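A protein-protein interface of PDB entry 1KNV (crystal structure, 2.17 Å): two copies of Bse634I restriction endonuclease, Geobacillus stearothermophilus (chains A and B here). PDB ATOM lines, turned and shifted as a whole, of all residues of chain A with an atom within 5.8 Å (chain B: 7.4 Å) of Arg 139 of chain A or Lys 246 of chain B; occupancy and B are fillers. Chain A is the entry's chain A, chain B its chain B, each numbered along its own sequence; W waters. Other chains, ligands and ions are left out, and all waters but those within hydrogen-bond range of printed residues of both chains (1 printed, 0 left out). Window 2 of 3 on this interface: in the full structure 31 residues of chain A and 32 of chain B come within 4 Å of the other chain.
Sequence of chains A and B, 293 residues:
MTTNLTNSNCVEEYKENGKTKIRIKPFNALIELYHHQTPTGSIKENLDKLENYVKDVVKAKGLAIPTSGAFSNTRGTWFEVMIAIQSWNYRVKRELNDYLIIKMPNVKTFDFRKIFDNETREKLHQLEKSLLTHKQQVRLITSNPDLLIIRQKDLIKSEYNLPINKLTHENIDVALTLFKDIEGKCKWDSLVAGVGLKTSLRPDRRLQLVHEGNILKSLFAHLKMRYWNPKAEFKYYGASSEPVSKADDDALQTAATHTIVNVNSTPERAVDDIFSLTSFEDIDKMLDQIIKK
The backbone carbonyl oxygen (O) of Gln 137 of chain A sits at hydrogen-bond distance from the guanidinium group (NE) of Arg 269 of chain B. N of Arg 139 of chain A lies within hydrogen-bond range of O of Gln 253 of chain B, at 2.9 Å. The guanidinium group (NH2) of Arg 139 of chain A lies within salt-bridge range of the side-chain carboxylate (OD2) of Asp 250 of chain B. N of Ala 255 of chain B lies within hydrogen-bond range of O of Arg 139 of chain A (2.9 Å).
Of the 16 printed residues of chain B, 8 touch a printed residue of chain A. Hydrophobic or aromatic side chains of chain B within 4 Å of the printed part of chain A: Ala 255. Of the 7 printed residues of chain A, 4 touch a printed residue of chain B. Hydrophobic or aromatic side chains of chain A within 4 Å of the printed part of chain B: Val 138 and Ile 141. Among the printed residues, Asp or Glu carboxylates within 4 Å of a Lys or Arg side-chain nitrogen of the other chain: Arg 139 of chain A with Asp 250 of chain B (3.3 Å).
No position is printed for both chains. Of the 12 pairs that touch across the chains among the printed residues, none has its exchanged pair printed and touching as well.
Among the printed residues, pairs that only touch across the chains: Val 138 of chain A with Ala 255 of chain B, Arg 139 of chain A with Thr 254 of chain B, Val 138 of chain A with Gln 253 of chain B, Ile 141 of chain A with Ala 251 of chain B, Gln 137 of chain A with Gln 253 of chain B, Val 138 of chain A with Glu 268 of chain B, Arg 139 of chain A with Lys 246 of chain B and Ile 141 of chain A with Asp 250 of chain B.
Of chain B, only Lys 246, Asp 250, Gln 253, Thr 254 and Ala 255 come within 4 Å of Arg 139 of chain A. Lys 246 of chain B touches just one residue of chain A: Arg 139 (3.9 Å). Printed residues of chain A within 4 Å of Glu 268 of chain B: Val 138. Printed residues of chain B within 4 Å of Gln 137 of chain A: Gln 253 and Arg 269. Printed residues of chain B within 4 Å of Val 138 of chain A: Gln 253, Ala 255 and Glu 268. Of the printed residues of chain A, Ala 255 of chain B touches Val 138 (3.2 Å) and Arg 139 (2.9 Å). Leu 252 of chain B touches none of the printed residues of chain A. The nearest printed residue of chain A that does not touch Lys 246 of chain B is Gln 137 of chain A (6.8 Å). The nearest printed residue of chain A that does not touch Gln 253 of chain B is Leu 132 of chain A (4.9 Å).
OD2 of Asp 250 of chain B lies within salt-bridge range of NZ of Lys 246 of chain B, 3.3 Å away. N of Ala 256 of chain B lies within hydrogen-bond range of O of Glu 268 of chain B. The backbone NH of Leu 132 of chain A sits at hydrogen-bond distance from the backbone carbonyl oxygen of Val 138 of chain A (3.3 Å).
Water W1 lies within hydrogen-bond range of the side-chain hydroxyl (OG1) of Thr 254 of chain B and the backbone NH (N) of Ile 141 of chain A.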
ATOM      1  N   LEU A 131      28.839  26.641 -11.316  1.00  0.00           N
ATOM      2  CA  LEU A 131      27.442  26.843 -11.640  1.00  0.00           C
ATOM      3  C   LEU A 131      26.701  27.416 -10.428  1.00  0.00           C
ATOM      4  O   LEU A 131      26.186  28.530 -10.500  1.00  0.00           O
ATOM      5  CB  LEU A 131      26.797  25.526 -12.089  1.00  0.00           C
ATOM      6  CG  LEU A 131      27.146  24.990 -13.462  1.00  0.00           C
ATOM      7  CD1 LEU A 131      26.365  23.710 -13.685  1.00  0.00           C
ATOM      8  CD2 LEU A 131      26.811  26.044 -14.478  1.00  0.00           C
ATOM      9  N   LEU A 132      26.712  26.690  -9.306  1.00  0.00           N
ATOM     10  CA  LEU A 132      26.038  27.123  -8.075  1.00  0.00           C
ATOM     11  C   LEU A 132      26.482  28.503  -7.566  1.00  0.00           C
ATOM     12  O   LEU A 132      25.744  29.130  -6.802  1.00  0.00           O
ATOM     13  CB  LEU A 132      26.232  26.085  -6.961  1.00  0.00           C
ATOM     14  CG  LEU A 132      25.490  24.754  -7.101  1.00  0.00           C
ATOM     15  CD1 LEU A 132      25.975  23.764  -6.040  1.00  0.00           C
ATOM     16  CD2 LEU A 132      23.998  25.016  -7.005  1.00  0.00           C
ATOM     17  N   GLN A 137      21.359  30.723  -8.743  1.00  0.00           N
ATOM     18  CA  GLN A 137      21.960  29.403  -8.747  1.00  0.00           C
ATOM     19  C   GLN A 137      21.441  28.514  -9.848  1.00  0.00           C
ATOM     20  O   GLN A 137      20.234  28.414 -10.089  1.00  0.00           O
ATOM     21  CB  GLN A 137      21.738  28.698  -7.421  1.00  0.00           C
ATOM     22  CG  GLN A 137      22.170  29.488  -6.228  1.00  0.00           C
ATOM     23  CD  GLN A 137      22.279  28.612  -5.009  1.00  0.00           C
ATOM     24  OE1 GLN A 137      21.421  27.752  -4.758  1.00  0.00           O
ATOM     25  NE2 GLN A 137      23.339  28.820  -4.237  1.00  0.00           N
ATOM     26  N   VAL A 138      22.389  27.868 -10.510  1.00  0.00           N
ATOM     27  CA  VAL A 138      22.114  26.938 -11.586  1.00  0.00           C
ATOM     28  C   VAL A 138      22.738  25.649 -11.102  1.00  0.00           C
ATOM     29  O   VAL A 138      23.935  25.603 -10.832  1.00  0.00           O
ATOM     30  CB  VAL A 138      22.814  27.367 -12.885  1.00  0.00           C
ATOM     31  CG1 VAL A 138      22.471  26.411 -13.992  1.00  0.00           C
ATOM     32  CG2 VAL A 138      22.406  28.780 -13.260  1.00  0.00           C
ATOM     33  N   ARG A 139      21.937  24.606 -10.959  1.00  0.00           N
ATOM     34  CA  ARG A 139      22.469  23.338 -10.498  1.00  0.00           C
ATOM     35  C   ARG A 139      22.682  22.357 -11.634  1.00  0.00           C
ATOM     36  O   ARG A 139      22.063  22.458 -12.688  1.00  0.00           O
ATOM     37  CB  ARG A 139      21.531  22.689  -9.482  1.00  0.00           C
ATOM     38  CG  ARG A 139      21.399  23.426  -8.180  1.00  0.00           C
ATOM     39  CD  ARG A 139      20.590  22.604  -7.190  1.00  0.00           C
ATOM     40  NE  ARG A 139      20.251  23.403  -6.014  1.00  0.00           N
ATOM     41  CZ  ARG A 139      19.560  22.953  -4.970  1.00  0.00           C
ATOM     42  NH1 ARG A 139      19.134  21.692  -4.950  1.00  0.00           N
ATOM     43  NH2 ARG A 139      19.277  23.765  -3.952  1.00  0.00           N
ATOM     44  N   LEU A 140      23.585  21.413 -11.408  1.00  0.00           N
ATOM     45  CA  LEU A 140      23.855  20.367 -12.370  1.00  0.00           C
ATOM     46  C   LEU A 140      23.116  19.156 -11.802  1.00  0.00           C
ATOM     47  O   LEU A 140      23.605  18.505 -10.894  1.00  0.00           O
ATOM     48  CB  LEU A 140      25.359  20.074 -12.450  1.00  0.00           C
ATOM     49  CG  LEU A 140      25.753  18.968 -13.436  1.00  0.00           C
ATOM     50  CD1 LEU A 140      25.346  19.396 -14.842  1.00  0.00           C
ATOM     51  CD2 LEU A 140      27.250  18.680 -13.362  1.00  0.00           C
ATOM     52  N   ILE A 141      21.916  18.879 -12.293  1.00  0.00           N
ATOM     53  CA  ILE A 141      21.171  17.738 -11.791  1.00  0.00           C
ATOM     54  C   ILE A 141      21.309  16.599 -12.783  1.00  0.00           C
ATOM     55  O   ILE A 141      21.038  16.766 -13.973  1.00  0.00           O
ATOM     56  CB  ILE A 141      19.684  18.079 -11.590  1.00  0.00           C
ATOM     57  CG1 ILE A 141      19.550  19.229 -10.586  1.00  0.00           C
ATOM     58  CG2 ILE A 141      18.923  16.843 -11.128  1.00  0.00           C
ATOM     59  CD1 ILE A 141      18.137  19.541 -10.210  1.00  0.00           C
ATOM     60  N   VAL B 244       4.347  26.269  -4.971  1.00  0.00           N
ATOM     61  CA  VAL B 244       5.578  25.602  -5.382  1.00  0.00           C
ATOM     62  C   VAL B 244       6.457  25.227  -4.185  1.00  0.00           C
ATOM     63  O   VAL B 244       6.860  26.086  -3.390  1.00  0.00           O
ATOM     64  CB  VAL B 244       6.391  26.488  -6.387  1.00  0.00           C
ATOM     65  CG1 VAL B 244       7.669  25.781  -6.820  1.00  0.00           C
ATOM     66  CG2 VAL B 244       5.544  26.794  -7.611  1.00  0.00           C
ATOM     67  N   SER B 245       6.740  23.933  -4.063  1.00  0.00           N
ATOM     68  CA  SER B 245       7.569  23.429  -2.975  1.00  0.00           C
ATOM     69  C   SER B 245       9.046  23.685  -3.254  1.00  0.00           C
ATOM     70  O   SER B 245       9.444  23.866  -4.402  1.00  0.00           O
ATOM     71  CB  SER B 245       7.345  21.929  -2.785  1.00  0.00           C
ATOM     72  OG  SER B 245       7.802  21.191  -3.904  1.00  0.00           O
ATOM     73  N   LYS B 246       9.855  23.689  -2.197  1.00  0.00           N
ATOM     74  CA  LYS B 246      11.290  23.919  -2.331  1.00  0.00           C
ATOM     75  C   LYS B 246      11.894  22.777  -3.140  1.00  0.00           C
ATOM     76  O   LYS B 246      12.832  22.976  -3.905  1.00  0.00           O
ATOM     77  CB  LYS B 246      11.945  23.986  -0.946  1.00  0.00           C
ATOM     78  CG  LYS B 246      13.165  24.915  -0.844  1.00  0.00           C
ATOM     79  CD  LYS B 246      14.502  24.154  -0.808  1.00  0.00           C
ATOM     80  CE  LYS B 246      15.691  25.121  -0.655  1.00  0.00           C
ATOM     81  NZ  LYS B 246      17.047  24.477  -0.790  1.00  0.00           N
ATOM     82  N   ALA B 247      11.343  21.578  -2.973  1.00  0.00           N
ATOM     83  CA  ALA B 247      11.839  20.418  -3.699  1.00  0.00           C
ATOM     84  C   ALA B 247      11.713  20.661  -5.196  1.00  0.00           C
ATOM     85  O   ALA B 247      12.654  20.426  -5.948  1.00  0.00           O
ATOM     86  CB  ALA B 247      11.067  19.170  -3.303  1.00  0.00           C
ATOM     87  N   ASP B 248      10.548  21.131  -5.625  1.00  0.00           N
ATOM     88  CA  ASP B 248      10.332  21.412  -7.036  1.00  0.00           C
ATOM     89  C   ASP B 248      11.143  22.617  -7.475  1.00  0.00           C
ATOM     90  O   ASP B 248      11.698  22.633  -8.565  1.00  0.00           O
ATOM     91  CB  ASP B 248       8.854  21.655  -7.321  1.00  0.00           C
ATOM     92  CG  ASP B 248       8.032  20.393  -7.208  1.00  0.00           C
ATOM     93  OD1 ASP B 248       8.537  19.319  -7.612  1.00  0.00           O
ATOM     94  OD2 ASP B 248       6.877  20.477  -6.730  1.00  0.00           O
ATOM     95  N   ASP B 249      11.215  23.631  -6.630  1.00  0.00           N
ATOM     96  CA  ASP B 249      11.987  24.801  -6.984  1.00  0.00           C
ATOM     97  C   ASP B 249      13.449  24.403  -7.176  1.00  0.00           C
ATOM     98  O   ASP B 249      14.112  24.857  -8.108  1.00  0.00           O
ATOM     99  CB  ASP B 249      11.887  25.855  -5.900  1.00  0.00           C
ATOM    100  CG  ASP B 249      12.400  27.190  -6.361  1.00  0.00           C
ATOM    101  OD1 ASP B 249      11.641  27.916  -7.042  1.00  0.00           O
ATOM    102  OD2 ASP B 249      13.576  27.497  -6.057  1.00  0.00           O
ATOM    103  N   ASP B 250      13.955  23.559  -6.282  1.00  0.00           N
ATOM    104  CA  ASP B 250      15.333  23.084  -6.373  1.00  0.00           C
ATOM    105  C   ASP B 250      15.555  22.404  -7.718  1.00  0.00           C
ATOM    106  O   ASP B 250      16.514  22.702  -8.431  1.00  0.00           O
ATOM    107  CB  ASP B 250      15.626  22.072  -5.256  1.00  0.00           C
ATOM    108  CG  ASP B 250      15.876  22.728  -3.903  1.00  0.00           C
ATOM    109  OD1 ASP B 250      15.956  21.976  -2.899  1.00  0.00           O
ATOM    110  OD2 ASP B 250      15.995  23.978  -3.840  1.00  0.00           O
ATOM    111  N   ALA B 251      14.657  21.477  -8.040  1.00  0.00           N
ATOM    112  CA  ALA B 251      14.725  20.723  -9.278  1.00  0.00           C
ATOM    113  C   ALA B 251      14.644  21.608 -10.510  1.00  0.00           C
ATOM    114  O   ALA B 251      15.258  21.298 -11.520  1.00  0.00           O
ATOM    115  CB  ALA B 251      13.614  19.690  -9.311  1.00  0.00           C
ATOM    116  N   LEU B 252      13.906  22.707 -10.415  1.00  0.00           N
ATOM    117  CA  LEU B 252      13.742  23.614 -11.544  1.00  0.00           C
ATOM    118  C   LEU B 252      14.931  24.582 -11.648  1.00  0.00           C
ATOM    119  O   LEU B 252      14.837  25.649 -12.256  1.00  0.00           O
ATOM    120  CB  LEU B 252      12.439  24.388 -11.416  1.00  0.00           C
ATOM    121  CG  LEU B 252      11.152  23.594 -11.611  1.00  0.00           C
ATOM    122  CD1 LEU B 252       9.946  24.493 -11.402  1.00  0.00           C
ATOM    123  CD2 LEU B 252      11.177  23.024 -13.005  1.00  0.00           C
ATOM    124  N   GLN B 253      16.064  24.185 -11.064  1.00  0.00           N
ATOM    125  CA  GLN B 253      17.300  24.979 -11.102  1.00  0.00           C
ATOM    126  C   GLN B 253      18.284  24.302 -12.049  1.00  0.00           C
ATOM    127  O   GLN B 253      19.368  24.810 -12.306  1.00  0.00           O
ATOM    128  CB  GLN B 253      17.935  25.104  -9.718  1.00  0.00           C
ATOM    129  CG  GLN B 253      17.294  26.140  -8.827  1.00  0.00           C
ATOM    130  CD  GLN B 253      17.976  26.226  -7.477  1.00  0.00           C
ATOM    131  OE1 GLN B 253      19.163  25.926  -7.324  1.00  0.00           O
ATOM    132  NE2 GLN B 253      17.224  26.658  -6.472  1.00  0.00           N
ATOM    133  N   THR B 254      17.875  23.156 -12.581  1.00  0.00           N
ATOM    134  CA  THR B 254      18.674  22.374 -13.515  1.00  0.00           C
ATOM    135  C   THR B 254      19.185  23.270 -14.660  1.00  0.00           C
ATOM    136  O   THR B 254      18.436  24.064 -15.236  1.00  0.00           O
ATOM    137  CB  THR B 254      17.828  21.189 -14.062  1.00  0.00           C
ATOM    138  OG1 THR B 254      18.594  20.424 -14.992  1.00  0.00           O
ATOM    139  CG2 THR B 254      16.588  21.692 -14.752  1.00  0.00           C
ATOM    140  N   ALA B 255      20.476  23.145 -14.962  1.00  0.00           N
ATOM    141  CA  ALA B 255      21.125  23.925 -16.009  1.00  0.00           C
ATOM    142  C   ALA B 255      20.724  23.541 -17.440  1.00  0.00           C
ATOM    143  O   ALA B 255      20.599  22.365 -17.770  1.00  0.00           O
ATOM    144  CB  ALA B 255      22.627  23.802 -15.857  1.00  0.00           C
ATOM    145  N   ALA B 256      20.525  24.537 -18.294  1.00  0.00           N
ATOM    146  CA  ALA B 256      20.189  24.267 -19.682  1.00  0.00           C
ATOM    147  C   ALA B 256      21.380  23.457 -20.193  1.00  0.00           C
ATOM    148  O   ALA B 256      22.511  23.930 -20.135  1.00  0.00           O
ATOM    149  CB  ALA B 256      20.064  25.584 -20.440  1.00  0.00           C
ATOM    150  N   ILE B 260      26.489  23.967 -20.863  1.00  0.00           N
ATOM    151  CA  ILE B 260      27.611  23.422 -20.096  1.00  0.00           C
ATOM    152  C   ILE B 260      28.738  22.826 -20.929  1.00  0.00           C
ATOM    153  O   ILE B 260      29.622  22.159 -20.390  1.00  0.00           O
ATOM    154  CB  ILE B 260      27.169  22.340 -19.065  1.00  0.00           C
ATOM    155  CG1 ILE B 260      26.663  21.083 -19.777  1.00  0.00           C
ATOM    156  CG2 ILE B 260      26.101  22.904 -18.141  1.00  0.00           C
ATOM    157  CD1 ILE B 260      26.403  19.913 -18.813  1.00  0.00           C
ATOM    158  N   GLU B 268      23.003  29.054 -17.296  1.00  0.00           N
ATOM    159  CA  GLU B 268      21.591  29.370 -17.166  1.00  0.00           C
ATOM    160  C   GLU B 268      20.727  28.138 -16.996  1.00  0.00           C
ATOM    161  O   GLU B 268      21.057  27.040 -17.459  1.00  0.00           O
ATOM    162  CB  GLU B 268      21.095  30.211 -18.348  1.00  0.00           C
ATOM    163  CG  GLU B 268      21.065  29.522 -19.676  1.00  0.00           C
ATOM    164  CD  GLU B 268      20.541  30.430 -20.777  1.00  0.00           C
ATOM    165  OE1 GLU B 268      19.374  30.864 -20.698  1.00  0.00           O
ATOM    166  OE2 GLU B 268      21.294  30.716 -21.725  1.00  0.00           O
ATOM    167  N   ARG B 269      19.623  28.328 -16.291  1.00  0.00           N
ATOM    168  CA  ARG B 269      18.685  27.258 -16.039  1.00  0.00           C
ATOM    169  C   ARG B 269      17.875  27.025 -17.300  1.00  0.00           C
ATOM    170  O   ARG B 269      17.744  27.908 -18.146  1.00  0.00           O
ATOM    171  CB  ARG B 269      17.714  27.659 -14.929  1.00  0.00           C
ATOM    172  CG  ARG B 269      18.344  28.161 -13.667  1.00  0.00           C
ATOM    173  CD  ARG B 269      17.258  28.602 -12.725  1.00  0.00           C
ATOM    174  NE  ARG B 269      17.782  28.957 -11.412  1.00  0.00           N
ATOM    175  CZ  ARG B 269      17.025  29.350 -10.385  1.00  0.00           C
ATOM    176  NH1 ARG B 269      15.703  29.438 -10.525  1.00  0.00           N
ATOM    177  NH2 ARG B 269      17.587  29.671  -9.221  1.00  0.00           N
HETATM  178  O   HOH W   1      21.120  19.577 -14.826  1.00  0.00           O
